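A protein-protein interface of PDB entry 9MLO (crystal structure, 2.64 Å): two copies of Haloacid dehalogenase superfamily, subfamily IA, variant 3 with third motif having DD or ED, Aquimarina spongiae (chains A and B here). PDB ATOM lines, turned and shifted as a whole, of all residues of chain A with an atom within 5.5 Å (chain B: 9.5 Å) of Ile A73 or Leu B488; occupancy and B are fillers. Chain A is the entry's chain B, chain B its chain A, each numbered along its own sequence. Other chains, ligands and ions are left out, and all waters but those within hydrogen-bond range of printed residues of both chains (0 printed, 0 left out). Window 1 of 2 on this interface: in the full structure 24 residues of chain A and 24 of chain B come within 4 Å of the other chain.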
ATOM      1  N   VAL A  64     -17.811  18.433 -20.678  1.00  0.00           N
ATOM      2  CA  VAL A  64     -17.898  19.683 -19.929  1.00  0.00           C
ATOM      3  C   VAL A  64     -19.288  20.282 -20.059  1.00  0.00           C
ATOM      4  O   VAL A  64     -19.765  20.972 -19.151  1.00  0.00           O
ATOM      5  CB  VAL A  64     -16.802  20.659 -20.402  1.00  0.00           C
ATOM      6  CG1 VAL A  64     -17.132  22.095 -20.033  1.00  0.00           C
ATOM      7  CG2 VAL A  64     -15.462  20.258 -19.821  1.00  0.00           C
ATOM      8  N   ASP A  67     -21.629  19.433 -17.166  1.00  0.00           N
ATOM      9  CA  ASP A  67     -21.506  20.293 -16.002  1.00  0.00           C
ATOM     10  C   ASP A  67     -22.323  21.564 -16.191  1.00  0.00           C
ATOM     11  O   ASP A  67     -23.019  22.014 -15.269  1.00  0.00           O
ATOM     12  CB  ASP A  67     -20.039  20.626 -15.744  1.00  0.00           C
ATOM     13  CG  ASP A  67     -19.207  19.406 -15.357  1.00  0.00           C
ATOM     14  OD1 ASP A  67     -19.648  18.577 -14.519  1.00  0.00           O
ATOM     15  OD2 ASP A  67     -18.082  19.293 -15.885  1.00  0.00           O
ATOM     16  N   LEU A  68     -22.255  22.151 -17.388  1.00  0.00           N
ATOM     17  CA  LEU A  68     -23.047  23.336 -17.684  1.00  0.00           C
ATOM     18  C   LEU A  68     -24.540  23.053 -17.542  1.00  0.00           C
ATOM     19  O   LEU A  68     -25.279  23.844 -16.946  1.00  0.00           O
ATOM     20  CB  LEU A  68     -22.711  23.838 -19.092  1.00  0.00           C
ATOM     21  CG  LEU A  68     -23.482  25.083 -19.522  1.00  0.00           C
ATOM     22  CD1 LEU A  68     -23.406  26.204 -18.459  1.00  0.00           C
ATOM     23  CD2 LEU A  68     -22.979  25.555 -20.844  1.00  0.00           C
ATOM     24  N   GLY A  71     -26.106  23.002 -14.030  1.00  0.00           N
ATOM     25  CA  GLY A  71     -25.895  24.187 -13.234  1.00  0.00           C
ATOM     26  C   GLY A  71     -24.640  24.225 -12.381  1.00  0.00           C
ATOM     27  O   GLY A  71     -24.505  25.146 -11.578  1.00  0.00           O
ATOM     28  N   LEU A  72     -23.701  23.286 -12.531  1.00  0.00           N
ATOM     29  CA  LEU A  72     -22.471  23.338 -11.736  1.00  0.00           C
ATOM     30  C   LEU A  72     -21.478  24.394 -12.224  1.00  0.00           C
ATOM     31  O   LEU A  72     -20.609  24.807 -11.453  1.00  0.00           O
ATOM     32  CB  LEU A  72     -21.782  21.974 -11.723  1.00  0.00           C
ATOM     33  CG  LEU A  72     -22.714  20.790 -11.484  1.00  0.00           C
ATOM     34  CD1 LEU A  72     -22.000  19.451 -11.673  1.00  0.00           C
ATOM     35  CD2 LEU A  72     -23.331  20.896 -10.111  1.00  0.00           C
ATOM     36  N   ILE A  73     -21.542  24.802 -13.490  1.00  0.00           N
ATOM     37  CA  ILE A  73     -20.711  25.882 -13.996  1.00  0.00           C
ATOM     38  C   ILE A  73     -21.592  26.766 -14.855  1.00  0.00           C
ATOM     39  O   ILE A  73     -22.648  26.352 -15.330  1.00  0.00           O
ATOM     40  CB  ILE A  73     -19.502  25.408 -14.825  1.00  0.00           C
ATOM     41  CG1 ILE A  73     -19.934  24.444 -15.930  1.00  0.00           C
ATOM     42  CG2 ILE A  73     -18.452  24.786 -13.953  1.00  0.00           C
ATOM     43  CD1 ILE A  73     -18.825  24.134 -16.911  1.00  0.00           C
ATOM     44  N   ASN A  74     -21.154  27.998 -15.053  1.00  0.00           N
ATOM     45  CA  ASN A  74     -21.895  28.865 -15.947  1.00  0.00           C
ATOM     46  C   ASN A  74     -21.270  28.817 -17.338  1.00  0.00           C
ATOM     47  O   ASN A  74     -20.302  28.096 -17.602  1.00  0.00           O
ATOM     48  CB  ASN A  74     -21.953  30.294 -15.411  1.00  0.00           C
ATOM     49  CG  ASN A  74     -20.591  30.928 -15.301  1.00  0.00           C
ATOM     50  OD1 ASN A  74     -19.706  30.414 -14.608  1.00  0.00           O
ATOM     51  ND2 ASN A  74     -20.406  32.044 -15.985  1.00  0.00           N
ATOM     52  N   GLN A  75     -21.841  29.610 -18.240  1.00  0.00           N
ATOM     53  CA  GLN A  75     -21.445  29.560 -19.635  1.00  0.00           C
ATOM     54  C   GLN A  75     -20.015  30.049 -19.824  1.00  0.00           C
ATOM     55  O   GLN A  75     -19.227  29.397 -20.511  1.00  0.00           O
ATOM     56  CB  GLN A  75     -22.428  30.372 -20.467  1.00  0.00           C
ATOM     57  CG  GLN A  75     -23.687  29.631 -20.775  1.00  0.00           C
ATOM     58  CD  GLN A  75     -24.427  30.212 -21.960  1.00  0.00           C
ATOM     59  OE1 GLN A  75     -23.974  31.175 -22.560  1.00  0.00           O
ATOM     60  NE2 GLN A  75     -25.571  29.627 -22.303  1.00  0.00           N
ATOM     61  N   PHE A  77     -17.477  29.959 -17.767  1.00  0.00           N
ATOM     62  CA  PHE A  77     -16.624  28.844 -17.399  1.00  0.00           C
ATOM     63  C   PHE A  77     -16.589  27.809 -18.498  1.00  0.00           C
ATOM     64  O   PHE A  77     -15.517  27.449 -18.983  1.00  0.00           O
ATOM     65  CB  PHE A  77     -17.117  28.207 -16.107  1.00  0.00           C
ATOM     66  CG  PHE A  77     -16.171  28.341 -14.995  1.00  0.00           C
ATOM     67  CD1 PHE A  77     -15.974  29.581 -14.410  1.00  0.00           C
ATOM     68  CD2 PHE A  77     -15.454  27.247 -14.537  1.00  0.00           C
ATOM     69  CE1 PHE A  77     -15.083  29.742 -13.378  1.00  0.00           C
ATOM     70  CE2 PHE A  77     -14.558  27.393 -13.501  1.00  0.00           C
ATOM     71  CZ  PHE A  77     -14.373  28.646 -12.915  1.00  0.00           C
ATOM     72  N   ALA A  78     -17.760  27.342 -18.925  1.00  0.00           N
ATOM     73  CA  ALA A  78     -17.826  26.243 -19.879  1.00  0.00           C
ATOM     74  C   ALA A  78     -17.118  26.591 -21.190  1.00  0.00           C
ATOM     75  O   ALA A  78     -16.422  25.752 -21.772  1.00  0.00           O
ATOM     76  CB  ALA A  78     -19.292  25.867 -20.109  1.00  0.00           C
ATOM     77  N   ALA A  81     -13.346  26.539 -20.774  1.00  0.00           N
ATOM     78  CA  ALA A  81     -12.817  25.188 -20.755  1.00  0.00           C
ATOM     79  C   ALA A  81     -12.835  24.576 -22.152  1.00  0.00           C
ATOM     80  O   ALA A  81     -11.850  23.946 -22.571  1.00  0.00           O
ATOM     81  CB  ALA A  81     -13.602  24.333 -19.760  1.00  0.00           C
ATOM     82  N   GLU A 133     -28.571  29.946 -18.135  1.00  0.00           N
ATOM     83  CA  GLU A 133     -28.610  31.164 -18.937  1.00  0.00           C
ATOM     84  C   GLU A 133     -29.400  30.965 -20.223  1.00  0.00           C
ATOM     85  O   GLU A 133     -30.064  31.893 -20.695  1.00  0.00           O
ATOM     86  CB  GLU A 133     -27.194  31.631 -19.237  1.00  0.00           C
ATOM     87  CG  GLU A 133     -26.393  31.919 -17.972  1.00  0.00           C
ATOM     88  CD  GLU A 133     -25.184  30.981 -17.784  1.00  0.00           C
ATOM     89  OE1 GLU A 133     -25.362  29.721 -17.649  1.00  0.00           O
ATOM     90  OE2 GLU A 133     -24.053  31.529 -17.778  1.00  0.00           O
ATOM     91  N   LYS B 231     -12.348   6.782  -8.600  1.00  0.00           N
ATOM     92  CA  LYS B 231     -12.869   7.115  -9.925  1.00  0.00           C
ATOM     93  C   LYS B 231     -12.364   8.477 -10.378  1.00  0.00           C
ATOM     94  O   LYS B 231     -11.799   8.612 -11.470  1.00  0.00           O
ATOM     95  CB  LYS B 231     -14.396   7.092  -9.915  1.00  0.00           C
ATOM     96  N   LYS B 232     -12.546   9.495  -9.533  1.00  0.00           N
ATOM     97  CA  LYS B 232     -12.155  10.853  -9.889  1.00  0.00           C
ATOM     98  C   LYS B 232     -10.652  10.969 -10.104  1.00  0.00           C
ATOM     99  O   LYS B 232     -10.203  11.747 -10.954  1.00  0.00           O
ATOM    100  CB  LYS B 232     -12.624  11.823  -8.807  1.00  0.00           C
ATOM    101  CG  LYS B 232     -14.134  11.996  -8.703  1.00  0.00           C
ATOM    102  CD  LYS B 232     -14.486  12.956  -7.565  1.00  0.00           C
ATOM    103  CE  LYS B 232     -15.893  13.525  -7.692  1.00  0.00           C
ATOM    104  NZ  LYS B 232     -15.943  14.754  -8.559  1.00  0.00           N
ATOM    105  N   LEU B 235      -9.967   9.294 -13.511  1.00  0.00           N
ATOM    106  CA  LEU B 235     -10.497  10.242 -14.480  1.00  0.00           C
ATOM    107  C   LEU B 235      -9.517  11.376 -14.733  1.00  0.00           C
ATOM    108  O   LEU B 235      -9.123  11.631 -15.876  1.00  0.00           O
ATOM    109  CB  LEU B 235     -11.825  10.797 -13.977  1.00  0.00           C
ATOM    110  CG  LEU B 235     -12.612  11.408 -15.117  1.00  0.00           C
ATOM    111  CD1 LEU B 235     -12.912  10.304 -16.099  1.00  0.00           C
ATOM    112  CD2 LEU B 235     -13.875  12.026 -14.607  1.00  0.00           C
ATOM    113  N   GLY B 236      -9.086  12.049 -13.663  1.00  0.00           N
ATOM    114  CA  GLY B 236      -8.245  13.221 -13.815  1.00  0.00           C
ATOM    115  C   GLY B 236      -6.852  12.903 -14.303  1.00  0.00           C
ATOM    116  O   GLY B 236      -6.235  13.712 -15.004  1.00  0.00           O
ATOM    117  N   TYR B 239      -7.246  12.624 -18.054  1.00  0.00           N
ATOM    118  CA  TYR B 239      -7.268  13.948 -18.675  1.00  0.00           C
ATOM    119  C   TYR B 239      -5.850  14.507 -18.827  1.00  0.00           C
ATOM    120  O   TYR B 239      -5.434  14.909 -19.924  1.00  0.00           O
ATOM    121  CB  TYR B 239      -8.139  14.919 -17.862  1.00  0.00           C
ATOM    122  CG  TYR B 239      -8.030  16.362 -18.358  1.00  0.00           C
ATOM    123  CD1 TYR B 239      -8.895  16.854 -19.344  1.00  0.00           C
ATOM    124  CD2 TYR B 239      -7.047  17.220 -17.865  1.00  0.00           C
ATOM    125  CE1 TYR B 239      -8.788  18.152 -19.813  1.00  0.00           C
ATOM    126  CE2 TYR B 239      -6.922  18.516 -18.337  1.00  0.00           C
ATOM    127  CZ  TYR B 239      -7.794  18.981 -19.308  1.00  0.00           C
ATOM    128  OH  TYR B 239      -7.668  20.278 -19.769  1.00  0.00           O
ATOM    129  N   ILE B 261     -11.072  33.911 -17.814  1.00  0.00           N
ATOM    130  CA  ILE B 261     -12.272  33.932 -18.631  1.00  0.00           C
ATOM    131  C   ILE B 261     -11.966  34.717 -19.902  1.00  0.00           C
ATOM    132  O   ILE B 261     -11.346  35.792 -19.856  1.00  0.00           O
ATOM    133  CB  ILE B 261     -13.453  34.503 -17.834  1.00  0.00           C
ATOM    134  CG1 ILE B 261     -14.388  33.372 -17.394  1.00  0.00           C
ATOM    135  CG2 ILE B 261     -14.239  35.482 -18.664  1.00  0.00           C
ATOM    136  CD1 ILE B 261     -13.759  32.331 -16.462  1.00  0.00           C
ATOM    137  N   PRO B 459      -9.436  25.720  -7.234  1.00  0.00           N
ATOM    138  CA  PRO B 459      -8.857  24.389  -6.986  1.00  0.00           C
ATOM    139  C   PRO B 459      -7.347  24.382  -6.827  1.00  0.00           C
ATOM    140  O   PRO B 459      -6.836  23.680  -5.948  1.00  0.00           O
ATOM    141  CB  PRO B 459      -9.307  23.597  -8.220  1.00  0.00           C
ATOM    142  CG  PRO B 459     -10.617  24.243  -8.605  1.00  0.00           C
ATOM    143  CD  PRO B 459     -10.401  25.709  -8.348  1.00  0.00           C
ATOM    144  N   LYS B 482     -13.653  19.777  -0.941  1.00  0.00           N
ATOM    145  CA  LYS B 482     -14.110  20.813  -1.858  1.00  0.00           C
ATOM    146  C   LYS B 482     -13.334  20.784  -3.184  1.00  0.00           C
ATOM    147  O   LYS B 482     -13.851  21.249  -4.204  1.00  0.00           O
ATOM    148  CB  LYS B 482     -14.011  22.181  -1.181  1.00  0.00           C
ATOM    149  N   LEU B 483     -12.121  20.220  -3.191  1.00  0.00           N
ATOM    150  CA  LEU B 483     -11.357  20.046  -4.422  1.00  0.00           C
ATOM    151  C   LEU B 483     -11.997  18.980  -5.307  1.00  0.00           C
ATOM    152  O   LEU B 483     -12.219  19.198  -6.504  1.00  0.00           O
ATOM    153  CB  LEU B 483      -9.914  19.678  -4.074  1.00  0.00           C
ATOM    154  CG  LEU B 483      -8.840  19.720  -5.147  1.00  0.00           C
ATOM    155  CD1 LEU B 483      -8.779  21.086  -5.693  1.00  0.00           C
ATOM    156  CD2 LEU B 483      -7.487  19.322  -4.591  1.00  0.00           C
ATOM    157  N   LEU B 484     -12.310  17.822  -4.726  1.00  0.00           N
ATOM    158  CA  LEU B 484     -13.089  16.813  -5.433  1.00  0.00           C
ATOM    159  C   LEU B 484     -14.312  17.409  -6.131  1.00  0.00           C
ATOM    160  O   LEU B 484     -14.643  17.018  -7.257  1.00  0.00           O
ATOM    161  CB  LEU B 484     -13.518  15.718  -4.458  1.00  0.00           C
ATOM    162  CG  LEU B 484     -12.410  15.094  -3.610  1.00  0.00           C
ATOM    163  CD1 LEU B 484     -12.970  13.970  -2.777  1.00  0.00           C
ATOM    164  CD2 LEU B 484     -11.280  14.593  -4.465  1.00  0.00           C
ATOM    165  N   ASP B 485     -14.984  18.372  -5.496  1.00  0.00           N
ATOM    166  CA  ASP B 485     -16.239  18.873  -6.053  1.00  0.00           C
ATOM    167  C   ASP B 485     -16.065  19.733  -7.302  1.00  0.00           C
ATOM    168  O   ASP B 485     -17.045  19.954  -8.022  1.00  0.00           O
ATOM    169  CB  ASP B 485     -16.999  19.698  -5.019  1.00  0.00           C
ATOM    170  CG  ASP B 485     -17.466  18.882  -3.850  1.00  0.00           C
ATOM    171  OD1 ASP B 485     -17.525  17.640  -3.975  1.00  0.00           O
ATOM    172  OD2 ASP B 485     -17.780  19.497  -2.806  1.00  0.00           O
ATOM    173  N   THR B 486     -14.872  20.258  -7.566  1.00  0.00           N
ATOM    174  CA  THR B 486     -14.705  21.245  -8.622  1.00  0.00           C
ATOM    175  C   THR B 486     -14.064  20.656  -9.870  1.00  0.00           C
ATOM    176  O   THR B 486     -13.708  21.401 -10.795  1.00  0.00           O
ATOM    177  CB  THR B 486     -13.907  22.433  -8.095  1.00  0.00           C
ATOM    178  OG1 THR B 486     -12.653  21.981  -7.576  1.00  0.00           O
ATOM    179  CG2 THR B 486     -14.676  23.080  -6.988  1.00  0.00           C
ATOM    180  N   GLN B 487     -13.932  19.335  -9.917  1.00  0.00           N
ATOM    181  CA  GLN B 487     -13.385  18.664 -11.080  1.00  0.00           C
ATOM    182  C   GLN B 487     -14.447  18.621 -12.161  1.00  0.00           C
ATOM    183  O   GLN B 487     -15.537  18.085 -11.935  1.00  0.00           O
ATOM    184  CB  GLN B 487     -12.947  17.252 -10.719  1.00  0.00           C
ATOM    185  CG  GLN B 487     -12.228  16.523 -11.826  1.00  0.00           C
ATOM    186  CD  GLN B 487     -12.041  15.038 -11.533  1.00  0.00           C
ATOM    187  OE1 GLN B 487     -12.906  14.403 -10.909  1.00  0.00           O
ATOM    188  NE2 GLN B 487     -10.917  14.472 -11.989  1.00  0.00           N
ATOM    189  N   LEU B 488     -14.133  19.174 -13.328  1.00  0.00           N
ATOM    190  CA  LEU B 488     -15.048  19.104 -14.450  1.00  0.00           C
ATOM    191  C   LEU B 488     -15.197  17.658 -14.927  1.00  0.00           C
ATOM    192  O   LEU B 488     -14.378  16.786 -14.623  1.00  0.00           O
ATOM    193  CB  LEU B 488     -14.562  20.004 -15.578  1.00  0.00           C
ATOM    194  CG  LEU B 488     -14.438  21.496 -15.248  1.00  0.00           C
ATOM    195  CD1 LEU B 488     -14.077  22.305 -16.508  1.00  0.00           C
ATOM    196  CD2 LEU B 488     -15.711  22.032 -14.577  1.00  0.00           C
ATOM    197  N   ALA B 489     -16.258  17.417 -15.703  1.00  0.00           N
ATOM    198  CA  ALA B 489     -16.697  16.064 -16.054  1.00  0.00           C
ATOM    199  C   ALA B 489     -15.728  15.307 -16.951  1.00  0.00           C
ATOM    200  O   ALA B 489     -15.812  14.078 -17.005  1.00  0.00           O
ATOM    201  CB  ALA B 489     -18.061  16.107 -16.741  1.00  0.00           C
ATOM    202  N   ASP B 490     -14.842  16.005 -17.673  1.00  0.00           N
ATOM    203  CA  ASP B 490     -13.835  15.417 -18.547  1.00  0.00           C
ATOM    204  C   ASP B 490     -12.572  15.030 -17.807  1.00  0.00           C
ATOM    205  O   ASP B 490     -11.604  14.612 -18.451  1.00  0.00           O
ATOM    206  CB  ASP B 490     -13.487  16.377 -19.699  1.00  0.00           C
ATOM    207  CG  ASP B 490     -12.786  17.665 -19.242  1.00  0.00           C
ATOM    208  OD1 ASP B 490     -12.628  17.879 -18.028  1.00  0.00           O
ATOM    209  OD2 ASP B 490     -12.388  18.478 -20.112  1.00  0.00           O
ATOM    210  N   GLY B 491     -12.555  15.189 -16.481  1.00  0.00           N
ATOM    211  CA  GLY B 491     -11.440  14.831 -15.653  1.00  0.00           C
ATOM    212  C   GLY B 491     -10.591  16.004 -15.208  1.00  0.00           C
ATOM    213  O   GLY B 491      -9.955  15.922 -14.154  1.00  0.00           O
ATOM    214  N   GLY B 492     -10.561  17.090 -15.981  1.00  0.00           N
ATOM    215  CA  GLY B 492      -9.702  18.210 -15.660  1.00  0.00           C
ATOM    216  C   GLY B 492     -10.354  19.233 -14.734  1.00  0.00           C
ATOM    217  O   GLY B 492     -11.574  19.327 -14.602  1.00  0.00           O
ATOM    218  N   TRP B 493      -9.524  19.999 -14.080  1.00  0.00           N
ATOM    219  CA  TRP B 493      -9.980  21.108 -13.265  1.00  0.00           C
ATOM    220  C   TRP B 493      -9.963  22.390 -14.087  1.00  0.00           C
ATOM    221  O   TRP B 493      -9.326  22.450 -15.135  1.00  0.00           O
ATOM    222  CB  TRP B 493      -9.092  21.230 -12.025  1.00  0.00           C
ATOM    223  CG  TRP B 493      -9.565  20.394 -10.859  1.00  0.00           C
ATOM    224  CD1 TRP B 493     -10.337  20.820  -9.814  1.00  0.00           C
ATOM    225  CD2 TRP B 493      -9.318  19.001 -10.627  1.00  0.00           C
ATOM    226  NE1 TRP B 493     -10.585  19.787  -8.942  1.00  0.00           N
ATOM    227  CE2 TRP B 493      -9.971  18.657  -9.408  1.00  0.00           C
ATOM    228  CE3 TRP B 493      -8.601  18.009 -11.313  1.00  0.00           C
ATOM    229  CZ2 TRP B 493      -9.928  17.354  -8.858  1.00  0.00           C
ATOM    230  CZ3 TRP B 493      -8.561  16.700 -10.760  1.00  0.00           C
ATOM    231  CH2 TRP B 493      -9.228  16.395  -9.545  1.00  0.00           C
ATOM    232  N   PRO B 494     -10.685  23.430 -13.664  1.00  0.00           N
ATOM    233  CA  PRO B 494     -10.708  24.680 -14.442  1.00  0.00           C
ATOM    234  C   PRO B 494      -9.341  25.334 -14.564  1.00  0.00           C
ATOM    235  O   PRO B 494      -8.469  25.170 -13.718  1.00  0.00           O
ATOM    236  CB  PRO B 494     -11.666  25.571 -13.639  1.00  0.00           C
ATOM    237  CG  PRO B 494     -12.583  24.605 -13.003  1.00  0.00           C
ATOM    238  CD  PRO B 494     -11.725  23.427 -12.618  1.00  0.00           C
ATOM    239  N   VAL B 495      -9.175  26.106 -15.642  1.00  0.00           N
ATOM    240  CA  VAL B 495      -7.954  26.873 -15.862  1.00  0.00           C
ATOM    241  C   VAL B 495      -7.740  27.832 -14.691  1.00  0.00           C
ATOM    242  O   VAL B 495      -8.693  28.227 -14.007  1.00  0.00           O
ATOM    243  CB  VAL B 495      -8.038  27.624 -17.207  1.00  0.00           C
ATOM    244  CG1 VAL B 495      -9.201  28.606 -17.209  1.00  0.00           C
ATOM    245  CG2 VAL B 495      -6.715  28.349 -17.552  1.00  0.00           C
ATOM    246  N   ARG B 511      -5.431  24.620 -17.794  1.00  0.00           N
ATOM    247  CA  ARG B 511      -6.114  23.561 -17.072  1.00  0.00           C
ATOM    248  C   ARG B 511      -5.145  22.455 -16.678  1.00  0.00           C
ATOM    249  O   ARG B 511      -5.457  21.637 -15.806  1.00  0.00           O
ATOM    250  CB  ARG B 511      -7.224  22.986 -17.944  1.00  0.00           C
ATOM    251  CG  ARG B 511      -8.262  23.962 -18.427  1.00  0.00           C
ATOM    252  CD  ARG B 511      -9.386  23.174 -19.099  1.00  0.00           C
ATOM    253  NE  ARG B 511      -9.995  22.198 -18.197  1.00  0.00           N
ATOM    254  CZ  ARG B 511     -10.823  21.228 -18.566  1.00  0.00           C
ATOM    255  NH1 ARG B 511     -11.143  21.037 -19.833  1.00  0.00           N
ATOM    256  NH2 ARG B 511     -11.337  20.421 -17.641  1.00  0.00           N
ATOM    257  N   SER B 514      -3.686  23.449 -13.180  1.00  0.00           N
ATOM    258  CA  SER B 514      -4.706  23.189 -12.168  1.00  0.00           C
ATOM    259  C   SER B 514      -4.852  21.697 -11.905  1.00  0.00           C
ATOM    260  O   SER B 514      -4.812  21.248 -10.753  1.00  0.00           O
ATOM    261  CB  SER B 514      -6.037  23.780 -12.610  1.00  0.00           C
ATOM    262  OG  SER B 514      -5.898  25.170 -12.756  1.00  0.00           O
ATOM    263  N   THR B 515      -5.031  20.915 -12.967  1.00  0.00           N
ATOM    264  CA  THR B 515      -5.182  19.477 -12.807  1.00  0.00           C
ATOM    265  C   THR B 515      -3.952  18.859 -12.162  1.00  0.00           C
ATOM    266  O   THR B 515      -4.071  17.907 -11.381  1.00  0.00           O
ATOM    267  CB  THR B 515      -5.450  18.840 -14.175  1.00  0.00           C
ATOM    268  OG1 THR B 515      -6.685  19.347 -14.699  1.00  0.00           O
ATOM    269  CG2 THR B 515      -5.522  17.334 -14.073  1.00  0.00           C
ATOM    270  N   ALA B 518      -4.020  19.490  -8.372  1.00  0.00           N
ATOM    271  CA  ALA B 518      -5.142  18.779  -7.769  1.00  0.00           C
ATOM    272  C   ALA B 518      -4.839  17.297  -7.628  1.00  0.00           C
ATOM    273  O   ALA B 518      -5.090  16.707  -6.574  1.00  0.00           O
ATOM    274  CB  ALA B 518      -6.410  18.994  -8.588  1.00  0.00           C
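Hydrophobic or aromatic side chains of chain B that line the printed part of chain A: Leu B488, Ala B489 and Pro B494. Among the printed residues, no Asp or Glu carboxylate lies within 4 Å of a Lys or Arg side-chain nitrogen of the other chain.
No position is printed for both chains.
Asp A67 touches two residues of chain B. No residue of chain B comes within 4 Å of Gly A71. Printed residues of chain B within 4 Å of Ile A73: Leu B488. Printed residues of chain B within 4 Å of Ala A81: Leu B488 (3.9 Å). Lys B231 touches none of the printed residues of chain A. Leu B488 touches just these residues of chain A: Asp A67 (3.4 Å), Ile A73 (3.9 Å) and Ala A81 (3.9 Å). Of the printed residues of chain A, Ala B489 touches Asp A67. Of the printed residues of chain A, Asp B490 touches Val A64. The nearest residue of chain B that does not touch Ile A73 is Pro B494 (5.9 Å). The nearest printed residue of chain A that does not touch Ala B489 is Val A64 (4.6 Å).
The backbone carbonyl oxygen of Asp A67 sits at hydrogen-bond distance from the backbone NH of Leu A72 (3.1 Å). OD1 of Asp B490 sits at hydrogen-bond distance from N of Gly B492, at 3.0 Å. OD2 of Asp B490 lies within salt-bridge range of NH1 of Arg B511 (2.9 Å). O of Pro B494 sits at hydrogen-bond distance from OG of Ser B514, at 2.7 Å.
OD2 of Asp A67 sits at hydrogen-bond distance from N of Ala B489.
Among the printed residues, pairs that only touch across the chains: Val A64 with Asp B490, Asp A67 with Leu B488, Ile A73 with Leu B488, Phe A77 with Pro B494 and Ala A81 with Leu B488.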
